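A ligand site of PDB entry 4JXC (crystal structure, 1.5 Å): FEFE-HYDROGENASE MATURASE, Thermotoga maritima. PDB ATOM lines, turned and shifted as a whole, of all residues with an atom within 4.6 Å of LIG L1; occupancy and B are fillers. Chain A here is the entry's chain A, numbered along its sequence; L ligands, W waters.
An iron atom (FE3) of LIG L1 is bound by the side-chain sulfur of Cys 63. SG of Cys 70 binds FE4 of LIG L1. The backbone NH of Cys 67 lies close to a sulfur (S2) of LIG L1, 3.8 Å away. The side-chain sulfur (SG) of Cys 67 binds an iron atom (FE1) of LIG L1 (2.3 Å). O of Tyr 69 is in hydrogen-bond range of N4 of LG2 L2 (2.9 Å). The backbone carbonyl oxygen (O) of Ser 108 lies close to a nitrogen (N1) of LG2 L2 (3.2 Å).
An iron atom (FE2) of LIG L1 is bound by an oxygen (O1) of LG2 L2 (2.3 Å).
N of Lys 65 sits close to SG of Cys 63 (3.4 Å). The side-chain sulfur of Cys 63 sits close to the backbone NH of Glu 110, at 3.3 Å. SG of Cys 70 sits close to N of Leu 72 (3.4 Å). The backbone carbonyl oxygen of Cys 67 lies within hydrogen-bond range of the guanidinium group of Arg 73, 3.0 Å away. SG of Cys 67 sits close to NE of Arg 172, at 3.6 Å. NE of Arg 172 sits at hydrogen-bond distance from OH of Tyr 69 (3.0 Å). The guanidinium group of Arg 73 sits at hydrogen-bond distance from the backbone carbonyl oxygen of Asn 66, at 2.9 Å. The side-chain amino group of Lys 65 is in salt-bridge range of the side-chain carboxylate of Glu 110 (2.7 Å).
CB of Lys 65 touches S4 of LIG L1 (3.9 Å). CE1 of Tyr 69 touches S3 of LIG L1, at 3.8 Å. CA of Arg 73 touches S2 of LIG L1, at 3.8 Å. Gly 109 touches LIG L1 (CA to S1, 3.7 Å). CG of Glu 110 touches S4 of LIG L1, at 3.96 Å. Eight residues have an atom within 4 Å of LIG L1: Cys 63, Lys 65, Cys 67, Tyr 69, Cys 70, Arg 73, Gly 109 and Glu 110. The nearest printed residue that does not touch LIG L1 is Leu 72 (4.1 Å).
Water W2 lies within hydrogen-bond range of OH of Tyr 69, NE of Arg 172 and S3 of LIG L1. Water W1 lies within hydrogen-bond range of OE2 of Glu 110 (2.7 Å), NH2 of Arg 172 (3.2 Å) and S4 of LIG L1 (3.3 Å).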
ATOM      1  N   CYS A  63       0.903 -16.231  -1.156  1.00  0.00           N
ATOM      2  CA  CYS A  63       2.303 -16.594  -1.075  1.00  0.00           C
ATOM      3  C   CYS A  63       2.550 -18.066  -0.784  1.00  0.00           C
ATOM      4  O   CYS A  63       1.906 -18.673   0.071  1.00  0.00           O
ATOM      5  CB  CYS A  63       3.045 -15.737  -0.035  1.00  0.00           C
ATOM      6  SG  CYS A  63       4.861 -15.792  -0.286  1.00  0.00           S
ATOM      7  N   LYS A  65       5.651 -19.040   0.190  1.00  0.00           N
ATOM      8  CA  LYS A  65       6.705 -19.111   1.216  1.00  0.00           C
ATOM      9  C   LYS A  65       6.152 -18.855   2.620  1.00  0.00           C
ATOM     10  O   LYS A  65       4.992 -18.453   2.778  1.00  0.00           O
ATOM     11  CB  LYS A  65       7.839 -18.152   0.883  1.00  0.00           C
ATOM     12  CG  LYS A  65       8.811 -18.705  -0.152  1.00  0.00           C
ATOM     13  CD  LYS A  65       9.994 -17.770  -0.365  1.00  0.00           C
ATOM     14  CE  LYS A  65      11.132 -18.417  -1.158  1.00  0.00           C
ATOM     15  NZ  LYS A  65      10.741 -18.944  -2.467  1.00  0.00           N
ATOM     16  N   ASN A  66       6.981 -19.101   3.631  1.00  0.00           N
ATOM     17  CA  ASN A  66       6.564 -19.131   5.020  1.00  0.00           C
ATOM     18  C   ASN A  66       7.446 -18.282   5.905  1.00  0.00           C
ATOM     19  O   ASN A  66       7.676 -18.643   7.066  1.00  0.00           O
ATOM     20  CB  ASN A  66       6.515 -20.598   5.521  1.00  0.00           C
ATOM     21  CG  ASN A  66       5.390 -20.861   6.507  1.00  0.00           C
ATOM     22  OD1 ASN A  66       4.432 -20.098   6.587  1.00  0.00           O
ATOM     23  ND2 ASN A  66       5.486 -21.972   7.237  1.00  0.00           N
ATOM     24  N   CYS A  67       7.932 -17.148   5.392  1.00  0.00           N
ATOM     25  CA  CYS A  67       8.869 -16.314   6.160  1.00  0.00           C
ATOM     26  C   CYS A  67       8.272 -16.022   7.523  1.00  0.00           C
ATOM     27  O   CYS A  67       7.102 -15.680   7.632  1.00  0.00           O
ATOM     28  CB  CYS A  67       9.240 -15.018   5.423  1.00  0.00           C
ATOM     29  SG  CYS A  67       9.784 -15.295   3.696  1.00  0.00           S
ATOM     30  N   TYR A  69       8.585 -13.710   9.690  1.00  0.00           N
ATOM     31  CA  TYR A  69       8.229 -12.328  10.016  1.00  0.00           C
ATOM     32  C   TYR A  69       6.973 -11.802   9.314  1.00  0.00           C
ATOM     33  O   TYR A  69       6.435 -10.775   9.737  1.00  0.00           O
ATOM     34  CB  TYR A  69       9.397 -11.379   9.717  1.00  0.00           C
ATOM     35  CG  TYR A  69      10.054 -11.605   8.383  1.00  0.00           C
ATOM     36  CD1 TYR A  69       9.496 -11.096   7.206  1.00  0.00           C
ATOM     37  CD2 TYR A  69      11.241 -12.366   8.262  1.00  0.00           C
ATOM     38  CE1 TYR A  69      10.107 -11.291   5.977  1.00  0.00           C
ATOM     39  CE2 TYR A  69      11.831 -12.583   7.036  1.00  0.00           C
ATOM     40  CZ  TYR A  69      11.244 -12.052   5.894  1.00  0.00           C
ATOM     41  OH  TYR A  69      11.854 -12.265   4.688  1.00  0.00           O
ATOM     42  N   CYS A  70       6.556 -12.452   8.245  1.00  0.00           N
ATOM     43  CA  CYS A  70       5.610 -11.843   7.295  1.00  0.00           C
ATOM     44  C   CYS A  70       4.156 -12.319   7.481  1.00  0.00           C
ATOM     45  O   CYS A  70       3.891 -13.522   7.487  1.00  0.00           O
ATOM     46  CB  CYS A  70       6.075 -12.148   5.877  1.00  0.00           C
ATOM     47  SG  CYS A  70       5.072 -11.355   4.609  1.00  0.00           S
ATOM     48  N   LEU A  72       1.877 -12.341   5.312  1.00  0.00           N
ATOM     49  CA  LEU A  72       1.413 -13.102   4.131  1.00  0.00           C
ATOM     50  C   LEU A  72       1.929 -14.556   4.084  1.00  0.00           C
ATOM     51  O   LEU A  72       1.565 -15.308   3.161  1.00  0.00           O
ATOM     52  CB  LEU A  72       1.797 -12.388   2.802  1.00  0.00           C
ATOM     53  CG  LEU A  72       1.538 -10.887   2.688  1.00  0.00           C
ATOM     54  CD1 LEU A  72       1.656 -10.451   1.220  1.00  0.00           C
ATOM     55  CD2 LEU A  72       0.200 -10.503   3.240  1.00  0.00           C
ATOM     56  N   ARG A  73       2.740 -14.967   5.068  1.00  0.00           N
ATOM     57  CA  ARG A  73       3.274 -16.320   5.071  1.00  0.00           C
ATOM     58  C   ARG A  73       2.179 -17.367   4.852  1.00  0.00           C
ATOM     59  O   ARG A  73       1.037 -17.189   5.314  1.00  0.00           O
ATOM     60  CB  ARG A  73       4.034 -16.578   6.368  1.00  0.00           C
ATOM     61  CG  ARG A  73       3.184 -16.623   7.617  1.00  0.00           C
ATOM     62  CD  ARG A  73       4.046 -16.489   8.867  1.00  0.00           C
ATOM     63  NE  ARG A  73       5.113 -17.454   8.905  1.00  0.00           N
ATOM     64  CZ  ARG A  73       5.075 -18.666   9.466  1.00  0.00           C
ATOM     65  NH1 ARG A  73       3.999 -19.119  10.115  1.00  0.00           N
ATOM     66  NH2 ARG A  73       6.131 -19.433   9.381  1.00  0.00           N
ATOM     67  N   SER A 108       3.983  -8.360  -4.944  1.00  0.00           N
ATOM     68  CA  SER A 108       3.083  -9.427  -4.505  1.00  0.00           C
ATOM     69  C   SER A 108       3.772 -10.377  -3.577  1.00  0.00           C
ATOM     70  O   SER A 108       4.999 -10.410  -3.461  1.00  0.00           O
ATOM     71  CB  SER A 108       2.540 -10.198  -5.708  1.00  0.00           C
ATOM     72  OG  SER A 108       3.591 -10.827  -6.457  1.00  0.00           O
ATOM     73  N   GLY A 109       2.962 -11.211  -2.927  1.00  0.00           N
ATOM     74  CA  GLY A 109       3.474 -12.480  -2.421  1.00  0.00           C
ATOM     75  C   GLY A 109       4.026 -13.301  -3.582  1.00  0.00           C
ATOM     76  O   GLY A 109       3.789 -12.986  -4.765  1.00  0.00           O
ATOM     77  N   GLU A 110       4.775 -14.339  -3.267  1.00  0.00           N
ATOM     78  CA  GLU A 110       5.242 -15.272  -4.286  1.00  0.00           C
ATOM     79  C   GLU A 110       4.067 -16.145  -4.689  1.00  0.00           C
ATOM     80  O   GLU A 110       3.886 -17.254  -4.197  1.00  0.00           O
ATOM     81  CB  GLU A 110       6.418 -16.125  -3.785  1.00  0.00           C
ATOM     82  CG  GLU A 110       7.675 -15.305  -3.572  1.00  0.00           C
ATOM     83  CD  GLU A 110       8.920 -16.170  -3.434  1.00  0.00           C
ATOM     84  OE1 GLU A 110       8.834 -17.407  -3.617  1.00  0.00           O
ATOM     85  OE2 GLU A 110      10.018 -15.605  -3.184  1.00  0.00           O
ATOM     86  N   ARG A 172      13.684 -17.560   7.027  1.00  0.00           N
ATOM     87  CA  ARG A 172      13.164 -17.781   5.678  1.00  0.00           C
ATOM     88  C   ARG A 172      13.430 -19.250   5.315  1.00  0.00           C
ATOM     89  O   ARG A 172      14.273 -19.567   4.470  1.00  0.00           O
ATOM     90  CB  ARG A 172      13.779 -16.776   4.697  1.00  0.00           C
ATOM     91  CG  ARG A 172      13.736 -15.336   5.199  1.00  0.00           C
ATOM     92  CD  ARG A 172      14.166 -14.321   4.146  1.00  0.00           C
ATOM     93  NE  ARG A 172      13.197 -14.326   3.058  1.00  0.00           N
ATOM     94  CZ  ARG A 172      13.428 -14.742   1.816  1.00  0.00           C
ATOM     95  NH1 ARG A 172      14.647 -15.075   1.401  1.00  0.00           N
ATOM     96  NH2 ARG A 172      12.396 -14.830   0.968  1.00  0.00           N
HETATM   97 FE1  LIG L   1       8.202 -14.056   2.491  1.00  0.00          FE
HETATM   98 FE2  LIG L   1       7.657 -12.085   0.505  1.00  0.00          FE
HETATM   99 FE3  LIG L   1       5.953 -14.309   0.976  1.00  0.00          FE
HETATM  100 FE4  LIG L   1       6.088 -12.390   2.870  1.00  0.00          FE
HETATM  101  S1  LIG L   1       5.327 -12.103   0.758  1.00  0.00           S
HETATM  102  S2  LIG L   1       6.097 -14.688   3.201  1.00  0.00           S
HETATM  103  S3  LIG L   1       8.290 -11.756   2.726  1.00  0.00           S
HETATM  104  S4  LIG L   1       8.148 -14.350   0.238  1.00  0.00           S
HETATM  105  N1  LG2 L   2       7.371 -11.554  -1.707  1.00  0.00           N
HETATM  106  C1  LG2 L   2       8.312 -10.501  -2.172  1.00  0.00           C
HETATM  107  C2  LG2 L   2       9.589 -10.605  -1.333  1.00  0.00           C
HETATM  108  O1  LG2 L   2       9.604 -11.237  -0.258  1.00  0.00           O
HETATM  109  O2  LG2 L   2      10.621 -10.067  -1.706  1.00  0.00           O
HETATM  110  C3  LG2 L   2       7.712  -9.107  -2.126  1.00  0.00           C
HETATM  111  C4  LG2 L   2       6.693  -8.846  -1.021  1.00  0.00           C
HETATM  112  S1  LG2 L   2       7.419  -8.874   0.635  1.00  0.00           S
HETATM  113  C5  LG2 L   2       5.901  -8.613   1.563  1.00  0.00           C
HETATM  114  C6  LG2 L   2       8.165  -7.193   0.704  1.00  0.00           C
HETATM  115  C7  LG2 L   2       9.066  -6.834   1.867  1.00  0.00           C
HETATM  116  O3  LG2 L   2       8.283  -6.687   3.048  1.00  0.00           O
HETATM  117  C8  LG2 L   2      10.127  -7.837   2.292  1.00  0.00           C
HETATM  118  O4  LG2 L   2      11.276  -7.760   1.460  1.00  0.00           O
HETATM  119  C9  LG2 L   2      10.363  -7.539   3.775  1.00  0.00           C
HETATM  120  O5  LG2 L   2      11.591  -6.857   3.965  1.00  0.00           O
HETATM  121  C10 LG2 L   2       9.162  -6.636   4.142  1.00  0.00           C
HETATM  122  N2  LG2 L   2       8.482  -7.199   5.314  1.00  0.00           N
HETATM  123  C11 LG2 L   2       7.824  -8.386   5.390  1.00  0.00           C
HETATM  124  N3  LG2 L   2       7.392  -8.557   6.654  1.00  0.00           N
HETATM  125  C12 LG2 L   2       7.784  -7.511   7.413  1.00  0.00           C
HETATM  126  C13 LG2 L   2       7.600  -7.158   8.742  1.00  0.00           C
HETATM  127  N4  LG2 L   2       6.958  -7.944   9.615  1.00  0.00           N
HETATM  128  N5  LG2 L   2       8.165  -5.967   9.162  1.00  0.00           N
HETATM  129  C14 LG2 L   2       8.823  -5.122   8.288  1.00  0.00           C
HETATM  130  N6  LG2 L   2       8.965  -5.461   6.985  1.00  0.00           N
HETATM  131  C15 LG2 L   2       8.454  -6.635   6.554  1.00  0.00           C
HETATM  132  O   HOH W   1      10.815 -13.631  -1.599  1.00  0.00           O
HETATM  133  O   HOH W   2      11.456 -11.877   2.020  1.00  0.00           O
